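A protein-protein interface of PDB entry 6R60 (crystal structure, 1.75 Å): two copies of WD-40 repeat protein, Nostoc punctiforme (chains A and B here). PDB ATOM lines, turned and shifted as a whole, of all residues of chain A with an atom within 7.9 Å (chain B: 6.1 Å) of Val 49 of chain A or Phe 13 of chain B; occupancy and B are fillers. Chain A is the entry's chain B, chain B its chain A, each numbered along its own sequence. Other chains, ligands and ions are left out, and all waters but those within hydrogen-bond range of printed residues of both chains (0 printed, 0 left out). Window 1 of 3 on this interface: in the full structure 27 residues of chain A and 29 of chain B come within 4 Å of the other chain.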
ATOM      1  N   GLN A  37      30.221 -29.489 -16.548  1.00  0.00           N
ATOM      2  CA  GLN A  37      29.201 -28.591 -17.107  1.00  0.00           C
ATOM      3  C   GLN A  37      28.965 -28.891 -18.568  1.00  0.00           C
ATOM      4  O   GLN A  37      27.817 -28.971 -18.990  1.00  0.00           O
ATOM      5  CB  GLN A  37      29.620 -27.108 -16.970  1.00  0.00           C
ATOM      6  CG  GLN A  37      28.496 -26.110 -17.014  1.00  0.00           C
ATOM      7  CD  GLN A  37      28.899 -24.801 -16.374  1.00  0.00           C
ATOM      8  OE1 GLN A  37      30.054 -24.385 -16.514  1.00  0.00           O
ATOM      9  NE2 GLN A  37      27.994 -24.153 -15.639  1.00  0.00           N
ATOM     10  N   GLN A  40      27.167 -32.182 -19.144  1.00  0.00           N
ATOM     11  CA  GLN A  40      25.787 -32.060 -18.708  1.00  0.00           C
ATOM     12  C   GLN A  40      24.970 -31.274 -19.731  1.00  0.00           C
ATOM     13  O   GLN A  40      23.793 -31.505 -19.900  1.00  0.00           O
ATOM     14  CB  GLN A  40      25.741 -31.375 -17.329  1.00  0.00           C
ATOM     15  CG  GLN A  40      24.349 -31.208 -16.709  1.00  0.00           C
ATOM     16  CD  GLN A  40      23.498 -32.470 -16.634  1.00  0.00           C
ATOM     17  OE1 GLN A  40      23.993 -33.615 -16.584  1.00  0.00           O
ATOM     18  NE2 GLN A  40      22.180 -32.269 -16.620  1.00  0.00           N
ATOM     19  N   HIS A  45      19.043 -32.814 -19.260  1.00  0.00           N
ATOM     20  CA  HIS A  45      17.605 -32.464 -19.458  1.00  0.00           C
ATOM     21  C   HIS A  45      17.239 -31.035 -19.086  1.00  0.00           C
ATOM     22  O   HIS A  45      17.900 -30.436 -18.263  1.00  0.00           O
ATOM     23  CB  HIS A  45      16.731 -33.439 -18.660  1.00  0.00           C
ATOM     24  CG  HIS A  45      16.684 -34.791 -19.283  1.00  0.00           C
ATOM     25  ND1 HIS A  45      15.993 -35.031 -20.449  1.00  0.00           N
ATOM     26  CD2 HIS A  45      17.283 -35.959 -18.951  1.00  0.00           C
ATOM     27  CE1 HIS A  45      16.134 -36.299 -20.793  1.00  0.00           C
ATOM     28  NE2 HIS A  45      16.910 -36.886 -19.897  1.00  0.00           N
ATOM     29  N   SER A  46      16.157 -30.509 -19.668  1.00  0.00           N
ATOM     30  CA  SER A  46      15.622 -29.169 -19.293  1.00  0.00           C
ATOM     31  C   SER A  46      15.597 -28.901 -17.790  1.00  0.00           C
ATOM     32  O   SER A  46      15.726 -27.747 -17.350  1.00  0.00           O
ATOM     33  CB  SER A  46      14.176 -28.986 -19.795  1.00  0.00           C
ATOM     34  OG  SER A  46      14.096 -29.077 -21.196  1.00  0.00           O
ATOM     35  N   SER A  47      15.393 -29.975 -17.018  1.00  0.00           N
ATOM     36  CA  SER A  47      15.231 -29.902 -15.565  1.00  0.00           C
ATOM     37  C   SER A  47      16.581 -29.954 -14.813  1.00  0.00           C
ATOM     38  O   SER A  47      16.600 -29.810 -13.591  1.00  0.00           O
ATOM     39  CB  SER A  47      14.276 -31.007 -15.056  1.00  0.00           C
ATOM     40  OG  SER A  47      14.766 -32.296 -15.361  1.00  0.00           O
ATOM     41  N   SER A  48      17.701 -30.152 -15.523  1.00  0.00           N
ATOM     42  CA  SER A  48      19.061 -30.058 -14.928  1.00  0.00           C
ATOM     43  C   SER A  48      19.203 -28.825 -14.051  1.00  0.00           C
ATOM     44  O   SER A  48      18.728 -27.735 -14.406  1.00  0.00           O
ATOM     45  CB  SER A  48      20.148 -29.988 -16.022  1.00  0.00           C
ATOM     46  OG  SER A  48      20.017 -31.045 -16.942  1.00  0.00           O
ATOM     47  N   VAL A  49      19.846 -29.000 -12.901  1.00  0.00           N
ATOM     48  CA  VAL A  49      19.860 -27.970 -11.872  1.00  0.00           C
ATOM     49  C   VAL A  49      21.196 -27.212 -11.908  1.00  0.00           C
ATOM     50  O   VAL A  49      22.269 -27.815 -11.833  1.00  0.00           O
ATOM     51  CB  VAL A  49      19.574 -28.586 -10.489  1.00  0.00           C
ATOM     52  CG1 VAL A  49      19.715 -27.552  -9.381  1.00  0.00           C
ATOM     53  CG2 VAL A  49      18.175 -29.197 -10.470  1.00  0.00           C
ATOM     54  N   TRP A  50      21.093 -25.885 -12.028  1.00  0.00           N
ATOM     55  CA  TRP A  50      22.231 -24.972 -12.202  1.00  0.00           C
ATOM     56  C   TRP A  50      22.463 -24.048 -10.971  1.00  0.00           C
ATOM     57  O   TRP A  50      23.420 -23.289 -10.968  1.00  0.00           O
ATOM     58  CB  TRP A  50      22.037 -24.164 -13.506  1.00  0.00           C
ATOM     59  CG  TRP A  50      22.234 -25.050 -14.720  1.00  0.00           C
ATOM     60  CD1 TRP A  50      21.447 -26.084 -15.041  1.00  0.00           C
ATOM     61  CD2 TRP A  50      23.297 -25.036 -15.708  1.00  0.00           C
ATOM     62  NE1 TRP A  50      21.914 -26.736 -16.159  1.00  0.00           N
ATOM     63  CE2 TRP A  50      23.052 -26.111 -16.588  1.00  0.00           C
ATOM     64  CE3 TRP A  50      24.420 -24.222 -15.938  1.00  0.00           C
ATOM     65  CZ2 TRP A  50      23.876 -26.397 -17.674  1.00  0.00           C
ATOM     66  CZ3 TRP A  50      25.234 -24.505 -17.028  1.00  0.00           C
ATOM     67  CH2 TRP A  50      24.961 -25.588 -17.876  1.00  0.00           C
ATOM     68  N   GLY A  51      21.613 -24.131  -9.934  1.00  0.00           N
ATOM     69  CA  GLY A  51      21.715 -23.263  -8.757  1.00  0.00           C
ATOM     70  C   GLY A  51      22.574 -23.801  -7.621  1.00  0.00           C
ATOM     71  O   GLY A  51      22.581 -23.282  -6.516  1.00  0.00           O
ATOM     72  N   VAL A  52      23.328 -24.847  -7.897  1.00  0.00           N
ATOM     73  CA  VAL A  52      24.351 -25.309  -6.933  1.00  0.00           C
ATOM     74  C   VAL A  52      25.631 -25.502  -7.710  1.00  0.00           C
ATOM     75  O   VAL A  52      25.600 -26.086  -8.780  1.00  0.00           O
ATOM     76  CB  VAL A  52      23.973 -26.656  -6.287  1.00  0.00           C
ATOM     77  CG1 VAL A  52      25.056 -27.110  -5.282  1.00  0.00           C
ATOM     78  CG2 VAL A  52      22.601 -26.553  -5.641  1.00  0.00           C
ATOM     79  N   ALA A  53      26.738 -25.051  -7.146  1.00  0.00           N
ATOM     80  CA  ALA A  53      28.037 -25.256  -7.751  1.00  0.00           C
ATOM     81  C   ALA A  53      29.048 -25.608  -6.669  1.00  0.00           C
ATOM     82  O   ALA A  53      28.908 -25.239  -5.496  1.00  0.00           O
ATOM     83  CB  ALA A  53      28.467 -24.000  -8.503  1.00  0.00           C
ATOM     84  N   PHE A  54      30.042 -26.354  -7.069  1.00  0.00           N
ATOM     85  CA  PHE A  54      31.139 -26.715  -6.212  1.00  0.00           C
ATOM     86  C   PHE A  54      32.376 -26.059  -6.764  1.00  0.00           C
ATOM     87  O   PHE A  54      32.540 -25.995  -7.972  1.00  0.00           O
ATOM     88  CB  PHE A  54      31.249 -28.227  -6.233  1.00  0.00           C
ATOM     89  CG  PHE A  54      29.945 -28.893  -5.865  1.00  0.00           C
ATOM     90  CD1 PHE A  54      29.512 -28.915  -4.551  1.00  0.00           C
ATOM     91  CD2 PHE A  54      29.096 -29.410  -6.854  1.00  0.00           C
ATOM     92  CE1 PHE A  54      28.294 -29.479  -4.209  1.00  0.00           C
ATOM     93  CE2 PHE A  54      27.868 -29.971  -6.517  1.00  0.00           C
ATOM     94  CZ  PHE A  54      27.464 -30.003  -5.194  1.00  0.00           C
ATOM     95  N   TRP A  91      18.864 -18.294  -9.883  1.00  0.00           N
ATOM     96  CA  TRP A  91      18.650 -19.646 -10.443  1.00  0.00           C
ATOM     97  C   TRP A  91      19.931 -20.401 -10.853  1.00  0.00           C
ATOM     98  O   TRP A  91      19.962 -21.650 -10.921  1.00  0.00           O
ATOM     99  CB  TRP A  91      17.823 -19.543 -11.690  1.00  0.00           C
ATOM    100  CG  TRP A  91      16.536 -18.795 -11.613  1.00  0.00           C
ATOM    101  CD1 TRP A  91      16.220 -17.674 -12.340  1.00  0.00           C
ATOM    102  CD2 TRP A  91      15.357 -19.137 -10.874  1.00  0.00           C
ATOM    103  NE1 TRP A  91      14.942 -17.293 -12.087  1.00  0.00           N
ATOM    104  CE2 TRP A  91      14.390 -18.155 -11.166  1.00  0.00           C
ATOM    105  CE3 TRP A  91      15.034 -20.157  -9.986  1.00  0.00           C
ATOM    106  CZ2 TRP A  91      13.108 -18.168 -10.611  1.00  0.00           C
ATOM    107  CZ3 TRP A  91      13.751 -20.169  -9.415  1.00  0.00           C
ATOM    108  CH2 TRP A  91      12.814 -19.181  -9.730  1.00  0.00           C
ATOM    109  N   GLY A  92      20.959 -19.653 -11.183  1.00  0.00           N
ATOM    110  CA  GLY A  92      22.226 -20.244 -11.675  1.00  0.00           C
ATOM    111  C   GLY A  92      23.413 -19.686 -10.935  1.00  0.00           C
ATOM    112  O   GLY A  92      23.425 -18.517 -10.546  1.00  0.00           O
ATOM    113  N   VAL A  93      24.399 -20.553 -10.657  1.00  0.00           N
ATOM    114  CA  VAL A  93      25.592 -20.137  -9.974  1.00  0.00           C
ATOM    115  C   VAL A  93      26.772 -20.856 -10.663  1.00  0.00           C
ATOM    116  O   VAL A  93      26.635 -22.055 -10.985  1.00  0.00           O
ATOM    117  CB  VAL A  93      25.550 -20.501  -8.459  1.00  0.00           C
ATOM    118  CG1 VAL A  93      26.757 -19.912  -7.742  1.00  0.00           C
ATOM    119  CG2 VAL A  93      24.283 -19.956  -7.843  1.00  0.00           C
ATOM    120  N   TRP A 132      18.998 -18.117 -16.468  1.00  0.00           N
ATOM    121  CA  TRP A 132      18.860 -19.436 -15.830  1.00  0.00           C
ATOM    122  C   TRP A 132      20.221 -20.009 -15.490  1.00  0.00           C
ATOM    123  O   TRP A 132      20.365 -20.730 -14.504  1.00  0.00           O
ATOM    124  CB  TRP A 132      18.139 -20.448 -16.750  1.00  0.00           C
ATOM    125  CG  TRP A 132      16.741 -20.070 -17.152  1.00  0.00           C
ATOM    126  CD1 TRP A 132      16.271 -19.957 -18.419  1.00  0.00           C
ATOM    127  CD2 TRP A 132      15.628 -19.784 -16.304  1.00  0.00           C
ATOM    128  NE1 TRP A 132      14.944 -19.598 -18.418  1.00  0.00           N
ATOM    129  CE2 TRP A 132      14.524 -19.496 -17.129  1.00  0.00           C
ATOM    130  CE3 TRP A 132      15.452 -19.738 -14.932  1.00  0.00           C
ATOM    131  CZ2 TRP A 132      13.262 -19.181 -16.623  1.00  0.00           C
ATOM    132  CZ3 TRP A 132      14.212 -19.414 -14.435  1.00  0.00           C
ATOM    133  CH2 TRP A 132      13.131 -19.128 -15.276  1.00  0.00           C
ATOM    134  N   TRP A 173      18.469 -23.140 -21.115  1.00  0.00           N
ATOM    135  CA  TRP A 173      18.656 -23.508 -19.752  1.00  0.00           C
ATOM    136  C   TRP A 173      20.094 -23.791 -19.313  1.00  0.00           C
ATOM    137  O   TRP A 173      20.390 -23.710 -18.108  1.00  0.00           O
ATOM    138  CB  TRP A 173      17.783 -24.727 -19.384  1.00  0.00           C
ATOM    139  CG  TRP A 173      18.001 -25.995 -20.211  1.00  0.00           C
ATOM    140  CD1 TRP A 173      17.247 -26.403 -21.237  1.00  0.00           C
ATOM    141  CD2 TRP A 173      19.021 -27.005 -20.026  1.00  0.00           C
ATOM    142  NE1 TRP A 173      17.708 -27.595 -21.730  1.00  0.00           N
ATOM    143  CE2 TRP A 173      18.785 -28.012 -20.979  1.00  0.00           C
ATOM    144  CE3 TRP A 173      20.099 -27.141 -19.153  1.00  0.00           C
ATOM    145  CZ2 TRP A 173      19.596 -29.160 -21.089  1.00  0.00           C
ATOM    146  CZ3 TRP A 173      20.926 -28.303 -19.255  1.00  0.00           C
ATOM    147  CH2 TRP A 173      20.666 -29.278 -20.229  1.00  0.00           C
ATOM    148  N   VAL B  11      30.598 -35.062  -4.281  1.00  0.00           N
ATOM    149  CA  VAL B  11      29.453 -34.142  -4.185  1.00  0.00           C
ATOM    150  C   VAL B  11      28.351 -34.596  -5.126  1.00  0.00           C
ATOM    151  O   VAL B  11      28.634 -35.256  -6.116  1.00  0.00           O
ATOM    152  CB  VAL B  11      29.863 -32.675  -4.540  1.00  0.00           C
ATOM    153  CG1 VAL B  11      30.777 -32.112  -3.460  1.00  0.00           C
ATOM    154  CG2 VAL B  11      30.550 -32.586  -5.899  1.00  0.00           C
ATOM    155  N   ALA B  12      27.101 -34.267  -4.807  1.00  0.00           N
ATOM    156  CA  ALA B  12      26.000 -34.463  -5.737  1.00  0.00           C
ATOM    157  C   ALA B  12      24.851 -33.567  -5.299  1.00  0.00           C
ATOM    158  O   ALA B  12      24.885 -32.949  -4.219  1.00  0.00           O
ATOM    159  CB  ALA B  12      25.569 -35.901  -5.750  1.00  0.00           C
ATOM    160  N   PHE B  13      23.858 -33.453  -6.162  1.00  0.00           N
ATOM    161  CA  PHE B  13      22.640 -32.801  -5.755  1.00  0.00           C
ATOM    162  C   PHE B  13      21.496 -33.616  -6.277  1.00  0.00           C
ATOM    163  O   PHE B  13      21.622 -34.293  -7.297  1.00  0.00           O
ATOM    164  CB  PHE B  13      22.607 -31.320  -6.179  1.00  0.00           C
ATOM    165  CG  PHE B  13      23.030 -31.099  -7.569  1.00  0.00           C
ATOM    166  CD1 PHE B  13      22.121 -31.267  -8.610  1.00  0.00           C
ATOM    167  CD2 PHE B  13      24.332 -30.736  -7.863  1.00  0.00           C
ATOM    168  CE1 PHE B  13      22.519 -31.093  -9.939  1.00  0.00           C
ATOM    169  CE2 PHE B  13      24.743 -30.555  -9.182  1.00  0.00           C
ATOM    170  CZ  PHE B  13      23.839 -30.734 -10.221  1.00  0.00           C
ATOM    171  N   SER B  14      20.390 -33.582  -5.550  1.00  0.00           N
ATOM    172  CA  SER B  14      19.241 -34.399  -5.888  1.00  0.00           C
ATOM    173  C   SER B  14      18.583 -33.940  -7.209  1.00  0.00           C
ATOM    174  O   SER B  14      18.738 -32.786  -7.614  1.00  0.00           O
ATOM    175  CB  SER B  14      18.225 -34.350  -4.754  1.00  0.00           C
ATOM    176  OG  SER B  14      17.792 -33.032  -4.495  1.00  0.00           O
ATOM    177  N   PRO B  15      17.883 -34.854  -7.910  1.00  0.00           N
ATOM    178  CA  PRO B  15      17.275 -34.465  -9.194  1.00  0.00           C
ATOM    179  C   PRO B  15      16.306 -33.273  -9.088  1.00  0.00           C
ATOM    180  O   PRO B  15      16.279 -32.426  -9.982  1.00  0.00           O
ATOM    181  CB  PRO B  15      16.592 -35.740  -9.646  1.00  0.00           C
ATOM    182  CG  PRO B  15      17.439 -36.827  -9.055  1.00  0.00           C
ATOM    183  CD  PRO B  15      17.872 -36.315  -7.713  1.00  0.00           C
ATOM    184  N   ASP B  16      15.595 -33.147  -7.969  1.00  0.00           N
ATOM    185  CA  ASP B  16      14.727 -31.978  -7.741  1.00  0.00           C
ATOM    186  C   ASP B  16      15.474 -30.726  -7.266  1.00  0.00           C
ATOM    187  O   ASP B  16      14.865 -29.682  -7.086  1.00  0.00           O
ATOM    188  CB  ASP B  16      13.564 -32.347  -6.811  1.00  0.00           C
ATOM    189  CG  ASP B  16      13.917 -32.309  -5.332  1.00  0.00           C
ATOM    190  OD1 ASP B  16      15.102 -32.253  -4.921  1.00  0.00           O
ATOM    191  OD2 ASP B  16      12.956 -32.362  -4.539  1.00  0.00           O
ATOM    192  N   GLY B  17      16.779 -30.855  -7.037  1.00  0.00           N
ATOM    193  CA  GLY B  17      17.675 -29.742  -6.728  1.00  0.00           C
ATOM    194  C   GLY B  17      17.663 -29.247  -5.296  1.00  0.00           C
ATOM    195  O   GLY B  17      18.426 -28.335  -4.969  1.00  0.00           O
ATOM    196  N   THR B  19      18.245 -30.966  -2.351  1.00  0.00           N
ATOM    197  CA  THR B  19      19.191 -31.556  -1.425  1.00  0.00           C
ATOM    198  C   THR B  19      20.570 -31.639  -2.033  1.00  0.00           C
ATOM    199  O   THR B  19      20.750 -32.089  -3.185  1.00  0.00           O
ATOM    200  CB  THR B  19      18.760 -32.960  -1.007  1.00  0.00           C
ATOM    201  OG1 THR B  19      17.408 -32.891  -0.506  1.00  0.00           O
ATOM    202  CG2 THR B  19      19.691 -33.474   0.090  1.00  0.00           C
ATOM    203  N   ILE B  20      21.544 -31.183  -1.250  1.00  0.00           N
ATOM    204  CA  ILE B  20      22.968 -31.208  -1.666  1.00  0.00           C
ATOM    205  C   ILE B  20      23.706 -32.215  -0.784  1.00  0.00           C
ATOM    206  O   ILE B  20      23.585 -32.147   0.416  1.00  0.00           O
ATOM    207  CB  ILE B  20      23.616 -29.823  -1.511  1.00  0.00           C
ATOM    208  CG1 ILE B  20      22.896 -28.786  -2.388  1.00  0.00           C
ATOM    209  CG2 ILE B  20      25.093 -29.864  -1.862  1.00  0.00           C
ATOM    210  CD1 ILE B  20      23.179 -27.363  -1.947  1.00  0.00           C
ATOM    211  N   ALA B  21      24.461 -33.125  -1.386  1.00  0.00           N
ATOM    212  CA  ALA B  21      25.269 -34.101  -0.636  1.00  0.00           C
ATOM    213  C   ALA B  21      26.726 -33.771  -0.819  1.00  0.00           C
ATOM    214  O   ALA B  21      27.175 -33.375  -1.922  1.00  0.00           O
ATOM    215  CB  ALA B  21      25.022 -35.510  -1.129  1.00  0.00           C
ATOM    216  N   ARG B  34      19.135 -26.071   0.440  1.00  0.00           N
ATOM    217  CA  ARG B  34      19.682 -25.025  -0.409  1.00  0.00           C
ATOM    218  C   ARG B  34      20.051 -23.721   0.337  1.00  0.00           C
ATOM    219  O   ARG B  34      20.689 -22.828  -0.251  1.00  0.00           O
ATOM    220  CB  ARG B  34      18.705 -24.756  -1.554  1.00  0.00           C
ATOM    221  CG  ARG B  34      18.641 -25.922  -2.546  1.00  0.00           C
ATOM    222  CD  ARG B  34      19.830 -25.871  -3.516  1.00  0.00           C
ATOM    223  NE  ARG B  34      19.762 -24.676  -4.332  1.00  0.00           N
ATOM    224  CZ  ARG B  34      19.108 -24.577  -5.480  1.00  0.00           C
ATOM    225  NH1 ARG B  34      19.050 -23.398  -6.104  1.00  0.00           N
ATOM    226  NH2 ARG B  34      18.486 -25.644  -6.010  1.00  0.00           N
ATOM    227  N   PHE B  54      22.582 -39.656  -6.278  1.00  0.00           N
ATOM    228  CA  PHE B  54      21.216 -39.841  -5.856  1.00  0.00           C
ATOM    229  C   PHE B  54      20.539 -40.725  -6.885  1.00  0.00           C
ATOM    230  O   PHE B  54      20.785 -40.622  -8.097  1.00  0.00           O
ATOM    231  CB  PHE B  54      20.455 -38.513  -5.811  1.00  0.00           C
ATOM    232  CG  PHE B  54      20.761 -37.646  -4.639  1.00  0.00           C
ATOM    233  CD1 PHE B  54      21.844 -36.813  -4.673  1.00  0.00           C
ATOM    234  CD2 PHE B  54      19.918 -37.612  -3.530  1.00  0.00           C
ATOM    235  CE1 PHE B  54      22.140 -35.985  -3.601  1.00  0.00           C
ATOM    236  CE2 PHE B  54      20.181 -36.758  -2.468  1.00  0.00           C
ATOM    237  CZ  PHE B  54      21.307 -35.961  -2.497  1.00  0.00           C
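Of the 12 printed residues of chain B, 6 touch a printed residue of chain A. Printed residues of chain B that touch a printed residue of chain A: Val 11, Phe 13, Pro 15, Gly 17, Ile 20 and Arg 34. Of the 17 printed residues of chain A, 4 touch a printed residue of chain B. Hydrophobic or aromatic side chains of chain A that line the printed part of chain B: Val 49, Val 52 and Phe 54. Among the printed residues, no Asp or Glu carboxylate lies within 4 Å of a Lys or Arg side-chain nitrogen of the other chain.
Among the printed residues, merely in contact across the chains: Val 49 of chain A with Phe 13 of chain B (3.7 Å), Val 49 of chain A with Pro 15 of chain B (3.8 Å), Val 49 of chain A with Gly 17 of chain B (3.8 Å), Gly 51 of chain A with Arg 34 of chain B (3.6 Å), Val 52 of chain A with Ile 20 of chain B (3.8 Å), Val 52 of chain A with Arg 34 of chain B (3.6 Å), Phe 54 of chain A with Val 11 of chain B (3.6 Å), Phe 54 of chain A with Phe 13 of chain B (3.9 Å) and Phe 54 of chain A with Ile 20 of chain B (3.99 Å).
N of Gly 17 of chain B lies within hydrogen-bond range of OG of Ser 14 of chain B (3.5 Å). O of Gly 17 of chain B is in hydrogen-bond range of NH2 of Arg 34 of chain B, 2.9 Å away. The backbone NH (N) of Gly 51 of chain A sits at hydrogen-bond distance from the backbone carbonyl oxygen (O) of Trp 91 of chain A (3.1 Å).
Position printed for both chains: 54. Of the 9 pairs that touch across the chains among the printed residues, none has its exchanged pair printed and touching as well.
Val 49 of chain A touches just these residues of chain B: Phe 13 (3.7 Å), Pro 15 (3.8 Å) and Gly 17 (3.8 Å). Of the printed residues of chain A, Val 11 of chain B touches Phe 54 (3.6 Å). Of the printed residues of chain A, Pro 15 of chain B touches Val 49 (3.8 Å).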
